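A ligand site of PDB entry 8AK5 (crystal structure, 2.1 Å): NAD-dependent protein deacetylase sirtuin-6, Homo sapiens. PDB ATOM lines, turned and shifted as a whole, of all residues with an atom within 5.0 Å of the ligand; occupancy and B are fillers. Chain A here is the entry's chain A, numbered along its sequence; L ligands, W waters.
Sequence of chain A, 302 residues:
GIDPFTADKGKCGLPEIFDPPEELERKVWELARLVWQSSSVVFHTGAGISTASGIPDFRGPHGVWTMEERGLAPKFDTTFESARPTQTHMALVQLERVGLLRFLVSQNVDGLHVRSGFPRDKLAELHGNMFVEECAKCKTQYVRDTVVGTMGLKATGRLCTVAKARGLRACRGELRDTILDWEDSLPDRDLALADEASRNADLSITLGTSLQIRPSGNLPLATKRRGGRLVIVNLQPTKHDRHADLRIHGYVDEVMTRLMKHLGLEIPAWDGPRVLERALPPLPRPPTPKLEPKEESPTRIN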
ATOM      1  N   GLU A  16     -23.156  -6.223  12.216  1.00  0.00           N
ATOM      2  CA  GLU A  16     -21.932  -5.654  11.624  1.00  0.00           C
ATOM      3  C   GLU A  16     -22.309  -4.902  10.343  1.00  0.00           C
ATOM      4  O   GLU A  16     -23.220  -5.340   9.624  1.00  0.00           O
ATOM      5  CB  GLU A  16     -20.906  -6.756  11.415  1.00  0.00           C
ATOM      6  CG  GLU A  16     -20.241  -7.171  12.719  1.00  0.00           C
ATOM      7  CD  GLU A  16     -19.320  -8.364  12.560  1.00  0.00           C
ATOM      8  OE1 GLU A  16     -19.541  -9.142  11.631  1.00  0.00           O
ATOM      9  OE2 GLU A  16     -18.401  -8.514  13.373  1.00  0.00           O
ATOM     10  N   GLY A  46      -9.886  -0.615  21.692  1.00  0.00           N
ATOM     11  CA  GLY A  46     -10.766  -1.523  22.422  1.00  0.00           C
ATOM     12  C   GLY A  46     -10.598  -2.898  21.805  1.00  0.00           C
ATOM     13  O   GLY A  46      -9.744  -3.051  20.858  1.00  0.00           O
ATOM     14  N   ALA A  47     -11.374  -3.826  22.321  1.00  0.00           N
ATOM     15  CA  ALA A  47     -11.122  -5.275  22.244  1.00  0.00           C
ATOM     16  C   ALA A  47     -11.042  -5.747  20.781  1.00  0.00           C
ATOM     17  O   ALA A  47     -10.487  -6.784  20.577  1.00  0.00           O
ATOM     18  CB  ALA A  47     -12.209  -5.970  23.020  1.00  0.00           C
ATOM     19  N   GLY A  48     -11.665  -5.005  19.858  1.00  0.00           N
ATOM     20  CA  GLY A  48     -11.707  -5.226  18.408  1.00  0.00           C
ATOM     21  C   GLY A  48     -10.346  -5.263  17.761  1.00  0.00           C
ATOM     22  O   GLY A  48     -10.197  -6.013  16.737  1.00  0.00           O
ATOM     23  N   THR A  51      -8.977  -9.208  18.143  1.00  0.00           N
ATOM     24  CA  THR A  51      -9.794 -10.383  17.773  1.00  0.00           C
ATOM     25  C   THR A  51      -9.014 -11.182  16.731  1.00  0.00           C
ATOM     26  O   THR A  51      -9.094 -12.411  16.786  1.00  0.00           O
ATOM     27  CB  THR A  51     -11.205 -10.007  17.316  1.00  0.00           C
ATOM     28  OG1 THR A  51     -11.095  -8.948  16.371  1.00  0.00           O
ATOM     29  CG2 THR A  51     -12.106  -9.565  18.444  1.00  0.00           C
ATOM     30  N   ASP A  57     -13.877 -10.290  21.681  1.00  0.00           N
ATOM     31  CA  ASP A  57     -14.246  -8.965  22.253  1.00  0.00           C
ATOM     32  C   ASP A  57     -15.427  -9.185  23.231  1.00  0.00           C
ATOM     33  O   ASP A  57     -15.670 -10.347  23.671  1.00  0.00           O
ATOM     34  CB  ASP A  57     -14.478  -7.956  21.121  1.00  0.00           C
ATOM     35  CG  ASP A  57     -15.618  -8.274  20.167  1.00  0.00           C
ATOM     36  OD1 ASP A  57     -16.467  -9.090  20.523  1.00  0.00           O
ATOM     37  OD2 ASP A  57     -15.656  -7.686  19.079  1.00  0.00           O
ATOM     38  N   PHE A  58     -16.095  -8.100  23.615  1.00  0.00           N
ATOM     39  CA  PHE A  58     -17.164  -8.145  24.633  1.00  0.00           C
ATOM     40  C   PHE A  58     -18.534  -8.154  23.937  1.00  0.00           C
ATOM     41  O   PHE A  58     -19.414  -8.882  24.372  1.00  0.00           O
ATOM     42  CB  PHE A  58     -16.953  -6.978  25.594  1.00  0.00           C
ATOM     43  CG  PHE A  58     -15.729  -7.205  26.445  1.00  0.00           C
ATOM     44  CD1 PHE A  58     -15.784  -8.031  27.556  1.00  0.00           C
ATOM     45  CD2 PHE A  58     -14.522  -6.594  26.145  1.00  0.00           C
ATOM     46  CE1 PHE A  58     -14.651  -8.275  28.307  1.00  0.00           C
ATOM     47  CE2 PHE A  58     -13.412  -6.797  26.922  1.00  0.00           C
ATOM     48  CZ  PHE A  58     -13.473  -7.660  27.999  1.00  0.00           C
ATOM     49  N   ARG A  59     -18.741  -7.290  22.935  1.00  0.00           N
ATOM     50  CA  ARG A  59     -20.106  -6.957  22.441  1.00  0.00           C
ATOM     51  C   ARG A  59     -20.247  -7.255  20.945  1.00  0.00           C
ATOM     52  O   ARG A  59     -21.312  -6.996  20.422  1.00  0.00           O
ATOM     53  CB  ARG A  59     -20.471  -5.519  22.799  1.00  0.00           C
ATOM     54  CG  ARG A  59     -20.389  -5.222  24.288  1.00  0.00           C
ATOM     55  CD  ARG A  59     -20.741  -3.790  24.672  1.00  0.00           C
ATOM     56  NE  ARG A  59     -20.556  -3.546  26.096  1.00  0.00           N
ATOM     57  CZ  ARG A  59     -19.380  -3.348  26.697  1.00  0.00           C
ATOM     58  NH1 ARG A  59     -18.252  -3.346  26.005  1.00  0.00           N
ATOM     59  NH2 ARG A  59     -19.329  -3.159  28.013  1.00  0.00           N
ATOM     60  N   GLY A  60     -19.250  -7.819  20.291  1.00  0.00           N
ATOM     61  CA  GLY A  60     -19.401  -8.273  18.888  1.00  0.00           C
ATOM     62  C   GLY A  60     -20.311  -9.494  18.829  1.00  0.00           C
ATOM     63  O   GLY A  60     -20.767  -9.992  19.856  1.00  0.00           O
ATOM     64  N   TRP A  65     -19.904 -10.845  26.576  1.00  0.00           N
ATOM     65  CA  TRP A  65     -21.266 -10.445  27.005  1.00  0.00           C
ATOM     66  C   TRP A  65     -22.306 -10.895  25.971  1.00  0.00           C
ATOM     67  O   TRP A  65     -23.387 -11.322  26.379  1.00  0.00           O
ATOM     68  CB  TRP A  65     -21.364  -8.944  27.275  1.00  0.00           C
ATOM     69  CG  TRP A  65     -20.321  -8.333  28.162  1.00  0.00           C
ATOM     70  CD1 TRP A  65     -19.914  -7.036  28.114  1.00  0.00           C
ATOM     71  CD2 TRP A  65     -19.616  -8.915  29.280  1.00  0.00           C
ATOM     72  NE1 TRP A  65     -18.968  -6.780  29.070  1.00  0.00           N
ATOM     73  CE2 TRP A  65     -18.765  -7.911  29.813  1.00  0.00           C
ATOM     74  CE3 TRP A  65     -19.592 -10.190  29.891  1.00  0.00           C
ATOM     75  CZ2 TRP A  65     -17.897  -8.137  30.884  1.00  0.00           C
ATOM     76  CZ3 TRP A  65     -18.740 -10.416  30.944  1.00  0.00           C
ATOM     77  CH2 TRP A  65     -17.909  -9.405  31.435  1.00  0.00           C
ATOM     78  N   GLN A 107      -8.701   0.640  26.482  1.00  0.00           N
ATOM     79  CA  GLN A 107      -9.575  -0.017  27.460  1.00  0.00           C
ATOM     80  C   GLN A 107      -9.231  -1.500  27.576  1.00  0.00           C
ATOM     81  O   GLN A 107      -9.898  -2.164  28.385  1.00  0.00           O
ATOM     82  CB  GLN A 107     -11.011   0.146  26.973  1.00  0.00           C
ATOM     83  CG  GLN A 107     -11.336   1.594  26.682  1.00  0.00           C
ATOM     84  CD  GLN A 107     -12.716   1.709  26.118  1.00  0.00           C
ATOM     85  OE1 GLN A 107     -13.704   1.402  26.786  1.00  0.00           O
ATOM     86  NE2 GLN A 107     -12.788   2.199  24.877  1.00  0.00           N
ATOM     87  N   ASN A 108      -8.249  -1.976  26.814  1.00  0.00           N
ATOM     88  CA  ASN A 108      -7.865  -3.417  26.790  1.00  0.00           C
ATOM     89  C   ASN A 108      -6.997  -3.764  27.976  1.00  0.00           C
ATOM     90  O   ASN A 108      -6.018  -3.068  28.204  1.00  0.00           O
ATOM     91  CB  ASN A 108      -7.074  -3.810  25.543  1.00  0.00           C
ATOM     92  CG  ASN A 108      -7.843  -3.465  24.294  1.00  0.00           C
ATOM     93  OD1 ASN A 108      -9.021  -3.180  24.398  1.00  0.00           O
ATOM     94  ND2 ASN A 108      -7.198  -3.442  23.140  1.00  0.00           N
ATOM     95  N   HIS A 127      -8.524   0.268  31.800  1.00  0.00           N
ATOM     96  CA  HIS A 127      -9.179  -0.838  32.544  1.00  0.00           C
ATOM     97  C   HIS A 127      -8.106  -1.749  33.132  1.00  0.00           C
ATOM     98  O   HIS A 127      -8.490  -2.771  33.700  1.00  0.00           O
ATOM     99  CB  HIS A 127     -10.206  -1.564  31.672  1.00  0.00           C
ATOM    100  CG  HIS A 127     -11.220  -0.615  31.109  1.00  0.00           C
ATOM    101  ND1 HIS A 127     -12.014  -0.927  30.019  1.00  0.00           N
ATOM    102  CD2 HIS A 127     -11.531   0.646  31.468  1.00  0.00           C
ATOM    103  CE1 HIS A 127     -12.805   0.107  29.758  1.00  0.00           C
ATOM    104  NE2 HIS A 127     -12.489   1.097  30.601  1.00  0.00           N
ATOM    105  N   TRP A 182     -16.234  -3.928  38.129  1.00  0.00           N
ATOM    106  CA  TRP A 182     -17.377  -3.075  37.712  1.00  0.00           C
ATOM    107  C   TRP A 182     -17.425  -1.746  38.493  1.00  0.00           C
ATOM    108  O   TRP A 182     -17.752  -0.727  37.871  1.00  0.00           O
ATOM    109  CB  TRP A 182     -18.684  -3.860  37.801  1.00  0.00           C
ATOM    110  CG  TRP A 182     -18.828  -4.852  36.685  1.00  0.00           C
ATOM    111  CD1 TRP A 182     -18.700  -6.211  36.767  1.00  0.00           C
ATOM    112  CD2 TRP A 182     -19.080  -4.550  35.302  1.00  0.00           C
ATOM    113  NE1 TRP A 182     -18.873  -6.780  35.530  1.00  0.00           N
ATOM    114  CE2 TRP A 182     -19.096  -5.787  34.606  1.00  0.00           C
ATOM    115  CE3 TRP A 182     -19.282  -3.368  34.577  1.00  0.00           C
ATOM    116  CZ2 TRP A 182     -19.329  -5.858  33.234  1.00  0.00           C
ATOM    117  CZ3 TRP A 182     -19.496  -3.433  33.216  1.00  0.00           C
ATOM    118  CH2 TRP A 182     -19.521  -4.674  32.555  1.00  0.00           C
ATOM    119  N   GLY A 208     -11.744  -0.528  16.961  1.00  0.00           N
ATOM    120  CA  GLY A 208     -12.284  -1.725  17.625  1.00  0.00           C
ATOM    121  C   GLY A 208     -12.820  -1.458  19.040  1.00  0.00           C
ATOM    122  O   GLY A 208     -12.715  -2.385  19.886  1.00  0.00           O
ATOM    123  N   THR A 209     -13.408  -0.283  19.311  1.00  0.00           N
ATOM    124  CA  THR A 209     -14.238  -0.037  20.526  1.00  0.00           C
ATOM    125  C   THR A 209     -15.661   0.400  20.104  1.00  0.00           C
ATOM    126  O   THR A 209     -15.800   1.069  19.078  1.00  0.00           O
ATOM    127  CB  THR A 209     -13.480   0.892  21.482  1.00  0.00           C
ATOM    128  OG1 THR A 209     -14.284   1.201  22.624  1.00  0.00           O
ATOM    129  CG2 THR A 209     -13.014   2.169  20.822  1.00  0.00           C
ATOM    130  N   SER A 210     -16.680  -0.093  20.818  1.00  0.00           N
ATOM    131  CA  SER A 210     -18.117   0.288  20.712  1.00  0.00           C
ATOM    132  C   SER A 210     -18.387   1.619  21.432  1.00  0.00           C
ATOM    133  O   SER A 210     -19.476   2.145  21.243  1.00  0.00           O
ATOM    134  CB  SER A 210     -18.969  -0.785  21.267  1.00  0.00           C
ATOM    135  OG  SER A 210     -18.528  -1.099  22.595  1.00  0.00           O
ATOM    136  N   LEU A 211     -17.463   2.118  22.250  1.00  0.00           N
ATOM    137  CA  LEU A 211     -17.517   3.479  22.866  1.00  0.00           C
ATOM    138  C   LEU A 211     -18.681   3.581  23.868  1.00  0.00           C
ATOM    139  O   LEU A 211     -19.220   4.673  24.071  1.00  0.00           O
ATOM    140  CB  LEU A 211     -17.586   4.542  21.768  1.00  0.00           C
ATOM    141  CG  LEU A 211     -16.301   4.682  20.962  1.00  0.00           C
ATOM    142  CD1 LEU A 211     -16.482   5.634  19.811  1.00  0.00           C
ATOM    143  CD2 LEU A 211     -15.157   5.118  21.868  1.00  0.00           C
ATOM    144  N   GLN A 212     -18.989   2.493  24.556  1.00  0.00           N
ATOM    145  CA  GLN A 212     -20.208   2.391  25.404  1.00  0.00           C
ATOM    146  C   GLN A 212     -19.898   2.603  26.898  1.00  0.00           C
ATOM    147  O   GLN A 212     -20.847   2.739  27.634  1.00  0.00           O
ATOM    148  CB  GLN A 212     -20.850   1.032  25.168  1.00  0.00           C
ATOM    149  CG  GLN A 212     -21.694   1.036  23.911  1.00  0.00           C
ATOM    150  CD  GLN A 212     -22.484  -0.241  23.887  1.00  0.00           C
ATOM    151  OE1 GLN A 212     -23.469  -0.394  24.606  1.00  0.00           O
ATOM    152  NE2 GLN A 212     -22.035  -1.185  23.071  1.00  0.00           N
ATOM    153  N   ILE A 213     -18.637   2.614  27.326  1.00  0.00           N
ATOM    154  CA  ILE A 213     -18.242   2.684  28.751  1.00  0.00           C
ATOM    155  C   ILE A 213     -17.811   4.116  29.076  1.00  0.00           C
ATOM    156  O   ILE A 213     -16.902   4.624  28.392  1.00  0.00           O
ATOM    157  CB  ILE A 213     -17.144   1.658  29.071  1.00  0.00           C
ATOM    158  CG1 ILE A 213     -17.625   0.217  28.860  1.00  0.00           C
ATOM    159  CG2 ILE A 213     -16.605   1.865  30.475  1.00  0.00           C
ATOM    160  CD1 ILE A 213     -18.386  -0.368  30.033  1.00  0.00           C
ATOM    161  N   VAL A 233     -13.294   3.731  13.685  1.00  0.00           N
ATOM    162  CA  VAL A 233     -13.053   2.498  12.875  1.00  0.00           C
ATOM    163  C   VAL A 233     -13.627   1.315  13.676  1.00  0.00           C
ATOM    164  O   VAL A 233     -13.151   1.037  14.760  1.00  0.00           O
ATOM    165  CB  VAL A 233     -11.563   2.359  12.540  1.00  0.00           C
ATOM    166  CG1 VAL A 233     -11.262   1.097  11.726  1.00  0.00           C
ATOM    167  CG2 VAL A 233     -11.056   3.574  11.771  1.00  0.00           C
ATOM    168  N   ASN A 234     -14.654   0.677  13.168  1.00  0.00           N
ATOM    169  CA  ASN A 234     -15.428  -0.327  13.932  1.00  0.00           C
ATOM    170  C   ASN A 234     -16.384  -1.039  12.988  1.00  0.00           C
ATOM    171  O   ASN A 234     -16.995  -0.346  12.204  1.00  0.00           O
ATOM    172  CB  ASN A 234     -16.236   0.317  15.063  1.00  0.00           C
ATOM    173  CG  ASN A 234     -16.400  -0.620  16.232  1.00  0.00           C
ATOM    174  OD1 ASN A 234     -15.432  -1.015  16.876  1.00  0.00           O
ATOM    175  ND2 ASN A 234     -17.629  -1.024  16.500  1.00  0.00           N
ATOM    176  N   LEU A 235     -16.517  -2.362  13.134  1.00  0.00           N
ATOM    177  CA  LEU A 235     -17.419  -3.220  12.327  1.00  0.00           C
ATOM    178  C   LEU A 235     -18.904  -2.981  12.683  1.00  0.00           C
ATOM    179  O   LEU A 235     -19.778  -3.204  11.821  1.00  0.00           O
ATOM    180  CB  LEU A 235     -17.058  -4.681  12.591  1.00  0.00           C
ATOM    181  CG  LEU A 235     -15.860  -5.214  11.814  1.00  0.00           C
ATOM    182  CD1 LEU A 235     -15.566  -6.642  12.234  1.00  0.00           C
ATOM    183  CD2 LEU A 235     -16.129  -5.153  10.311  1.00  0.00           C
ATOM    184  N   GLN A 236     -19.174  -2.579  13.923  1.00  0.00           N
ATOM    185  CA  GLN A 236     -20.529  -2.358  14.458  1.00  0.00           C
ATOM    186  C   GLN A 236     -20.713  -0.859  14.657  1.00  0.00           C
ATOM    187  O   GLN A 236     -19.734  -0.132  14.816  1.00  0.00           O
ATOM    188  CB  GLN A 236     -20.691  -3.040  15.807  1.00  0.00           C
ATOM    189  CG  GLN A 236     -20.726  -4.547  15.732  1.00  0.00           C
ATOM    190  CD  GLN A 236     -20.964  -5.112  17.103  1.00  0.00           C
ATOM    191  OE1 GLN A 236     -20.595  -4.504  18.112  1.00  0.00           O
ATOM    192  NE2 GLN A 236     -21.588  -6.274  17.166  1.00  0.00           N
ATOM    193  N   PRO A 237     -21.989  -0.400  14.728  1.00  0.00           N
ATOM    194  CA  PRO A 237     -22.273   0.964  15.186  1.00  0.00           C
ATOM    195  C   PRO A 237     -21.535   1.129  16.525  1.00  0.00           C
ATOM    196  O   PRO A 237     -21.196   0.117  17.062  1.00  0.00           O
ATOM    197  CB  PRO A 237     -23.795   0.987  15.437  1.00  0.00           C
ATOM    198  CG  PRO A 237     -24.340  -0.211  14.675  1.00  0.00           C
ATOM    199  CD  PRO A 237     -23.194  -1.186  14.454  1.00  0.00           C
ATOM    200  N   GLY A 250     -14.963  -1.726   8.707  1.00  0.00           N
ATOM    201  CA  GLY A 250     -14.130  -2.818   8.195  1.00  0.00           C
ATOM    202  C   GLY A 250     -13.208  -3.314   9.269  1.00  0.00           C
ATOM    203  O   GLY A 250     -13.162  -2.689  10.374  1.00  0.00           O
ATOM    204  N   TYR A 251     -12.489  -4.399   8.970  1.00  0.00           N
ATOM    205  CA  TYR A 251     -11.459  -4.963   9.872  1.00  0.00           C
ATOM    206  C   TYR A 251     -10.355  -3.942  10.070  1.00  0.00           C
ATOM    207  O   TYR A 251      -9.913  -3.379   9.041  1.00  0.00           O
ATOM    208  CB  TYR A 251     -10.934  -6.260   9.269  1.00  0.00           C
ATOM    209  CG  TYR A 251     -12.045  -7.249   9.110  1.00  0.00           C
ATOM    210  CD1 TYR A 251     -12.477  -7.996  10.188  1.00  0.00           C
ATOM    211  CD2 TYR A 251     -12.690  -7.409   7.903  1.00  0.00           C
ATOM    212  CE1 TYR A 251     -13.492  -8.924  10.047  1.00  0.00           C
ATOM    213  CE2 TYR A 251     -13.723  -8.322   7.756  1.00  0.00           C
ATOM    214  CZ  TYR A 251     -14.097  -9.103   8.837  1.00  0.00           C
ATOM    215  OH  TYR A 251     -15.115 -10.001   8.721  1.00  0.00           O
ATOM    216  N   VAL A 252      -9.924  -3.739  11.323  1.00  0.00           N
ATOM    217  CA  VAL A 252      -8.910  -2.684  11.642  1.00  0.00           C
ATOM    218  C   VAL A 252      -7.568  -3.074  11.010  1.00  0.00           C
ATOM    219  O   VAL A 252      -6.870  -2.197  10.452  1.00  0.00           O
ATOM    220  CB  VAL A 252      -8.818  -2.422  13.159  1.00  0.00           C
ATOM    221  CG1 VAL A 252     -10.062  -1.698  13.622  1.00  0.00           C
ATOM    222  CG2 VAL A 252      -8.611  -3.683  13.995  1.00  0.00           C
HETATM  223  N1  LIG L   1     -11.979  -4.921  13.191  1.00  0.00           N
HETATM  224  C1  LIG L   1     -12.769  -3.910  13.538  1.00  0.00           C
HETATM  225  N2  LIG L   1     -13.679  -3.842  14.503  1.00  0.00           N
HETATM  226  C2  LIG L   1     -13.727  -4.998  15.165  1.00  0.00           C
HETATM  227  C3  LIG L   1     -12.978  -6.133  14.929  1.00  0.00           C
HETATM  228  C4  LIG L   1     -12.043  -6.081  13.872  1.00  0.00           C
HETATM  229  N3  LIG L   1     -11.191  -7.041  13.549  1.00  0.00           N
HETATM  230  N4  LIG L   1     -13.331  -7.121  15.838  1.00  0.00           N
HETATM  231  C5  LIG L   1     -14.258  -6.581  16.577  1.00  0.00           C
HETATM  232  N5  LIG L   1     -14.568  -5.305  16.197  1.00  0.00           N
HETATM  233  P1  LIG L   1     -16.600  -4.027  22.656  1.00  0.00           P
HETATM  234  P2  LIG L   1     -14.703  -2.434  24.181  1.00  0.00           P
HETATM  235  C6  LIG L   1     -15.510  -4.364  16.829  1.00  0.00           C
HETATM  236  O1  LIG L   1     -17.628  -3.347  23.482  1.00  0.00           O
HETATM  237  O2  LIG L   1     -13.201  -2.385  24.123  1.00  0.00           O
HETATM  238  C7  LIG L   1     -16.030  -4.251  28.865  1.00  0.00           C
HETATM  239  O3  LIG L   1     -16.949  -4.395  29.862  1.00  0.00           O
HETATM  240  C8  LIG L   1     -16.812  -4.978  17.340  1.00  0.00           C
HETATM  241  O4  LIG L   1     -17.728  -4.954  16.255  1.00  0.00           O
HETATM  242  O5  LIG L   1     -16.702  -5.492  22.334  1.00  0.00           O
HETATM  243  O6  LIG L   1     -15.465  -1.281  23.608  1.00  0.00           O
HETATM  244  C9  LIG L   1     -14.567  -4.275  29.345  1.00  0.00           C
HETATM  245  O7  LIG L   1     -14.391  -3.525  30.521  1.00  0.00           O
HETATM  246  C10 LIG L   1     -17.177  -4.041  18.521  1.00  0.00           C
HETATM  247  O8  LIG L   1     -18.025  -2.972  18.133  1.00  0.00           O
HETATM  248  O9  LIG L   1     -15.207  -3.779  23.443  1.00  0.00           O
HETATM  249  C11 LIG L   1     -13.876  -3.545  28.177  1.00  0.00           C
HETATM  250  O10 LIG L   1     -12.609  -2.952  28.456  1.00  0.00           O
HETATM  251  C12 LIG L   1     -15.852  -3.402  18.955  1.00  0.00           C
HETATM  252  O11 LIG L   1     -14.872  -3.836  17.970  1.00  0.00           O
HETATM  253  C13 LIG L   1     -14.868  -2.403  27.981  1.00  0.00           C
HETATM  254  O12 LIG L   1     -16.175  -2.947  28.251  1.00  0.00           O
HETATM  255  C14 LIG L   1     -15.363  -3.740  20.333  1.00  0.00           C
HETATM  256  O13 LIG L   1     -16.294  -3.204  21.328  1.00  0.00           O
HETATM  257  C15 LIG L   1     -14.872  -1.744  26.623  1.00  0.00           C
HETATM  258  O14 LIG L   1     -15.209  -2.746  25.652  1.00  0.00           O
HETATM  259  O   HOH W   1     -16.951   0.730  25.160  1.00  0.00           O
HETATM  260  O   HOH W   2      -8.618  -7.307  11.778  1.00  0.00           O
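The side-chain amide nitrogen (NE2) of Gln 107 sits at hydrogen-bond distance from the side-chain hydroxyl (OG1) of Thr 209 (2.9 Å).
The backbone carbonyl oxygen (O) of Gly 208 is in hydrogen-bond range of the backbone NH (N) of Gly 48 (2.8 Å).
OG1 of Thr 209 lies close to N of Leu 211, at 3.3 Å.
O of Gly 48 sits at hydrogen-bond distance from OG1 of Thr 51 (3.1 Å).
The side-chain carboxylate (OD1) of Asp 57 lies within hydrogen-bond range of the backbone NH (N) of Gly 60 (3.1 Å).
The backbone carbonyl oxygen (O) of Phe 58 is in hydrogen-bond range of the backbone NH (N) of Trp 65 (3.0 Å).
The backbone carbonyl oxygen (O) of Arg 59 lies within hydrogen-bond range of the side-chain amide nitrogen (NE2) of Gln 236, 3.3 Å away.
OD1 of Asn 234 sits close to O of Thr 209 (3.1 Å).
An oxygen (O11) of the ligand sits close to the backbone carbonyl oxygen (O) of Gly 208.
CA of Gly 46 touches O2 of the ligand, at 3.1 Å.
Asp 57 touches the ligand (OD2 to C5, 3.1 Å).
Trp 182 touches the ligand (CH2 to O3, 3.7 Å).
Ile 213 touches the ligand.
Gly 250 touches the ligand.
Tyr 251 touches the ligand (CA to N1, 3.4 Å).
Hydrophobic or aromatic side chains that line the ligand: Ala 47, Phe 58, Trp 65, His 127, Trp 182, Ile 213, Leu 235, Tyr 251 and Val 252.
21 residues have an atom within 4 Å of the ligand: Gly 46, Ala 47, Gly 48, Thr 51, Asp 57, Phe 58, Arg 59, Trp 65, Gln 107, His 127, Trp 182, Gly 208, Thr 209, Ser 210, Ile 213, Asn 234, Leu 235, Gln 236, Gly 250, Tyr 251 and Val 252.
The side-chain hydroxyl (OG) of Ser 210 lies within hydrogen-bond range of an oxygen (O1) of the ligand (2.6 Å).
An oxygen (O8) of the ligand is in hydrogen-bond range of the side-chain amide oxygen (OE1) of Gln 236.
NH1 of Arg 59 is in salt-bridge range of O1 of the ligand (2.6 Å).
The backbone NH of Ala 47 is in hydrogen-bond range of an oxygen (O2) of the ligand (2.9 Å).
An oxygen (O8) of the ligand sits at hydrogen-bond distance from the side-chain amide nitrogen of Asn 234.
N4 of the ligand sits at hydrogen-bond distance from OG1 of Thr 51, 2.9 Å away.
An oxygen (O5) of the ligand sits at hydrogen-bond distance from the backbone NH (N) of Phe 58, at 3.0 Å.
The backbone NH (N) of Arg 59 is in hydrogen-bond range of an oxygen (O5) of the ligand (2.8 Å).
The backbone carbonyl oxygen (O) of Gln 107 lies within hydrogen-bond range of an oxygen (O10) of the ligand (2.8 Å).
An oxygen (O6) of the ligand sits at hydrogen-bond distance from the side-chain hydroxyl of Thr 209, at 2.9 Å.
ND1 of His 127 lies within hydrogen-bond range of O10 of the ligand (2.6 Å).
The backbone NH of Leu 235 lies within hydrogen-bond range of a nitrogen (N2) of the ligand, at 3.5 Å.
The backbone carbonyl oxygen (O) of Gly 48 lies close to a nitrogen (N3) of the ligand, 3.5 Å away.
The backbone NH (N) of Ser 210 lies within hydrogen-bond range of an oxygen (O13) of the ligand (3.2 Å).
An oxygen (O3) of the ligand lies within hydrogen-bond range of the indole nitrogen (NE1) of Trp 65, 3.2 Å away.
N1 of the ligand is in hydrogen-bond range of N of Val 252 (3.0 Å).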
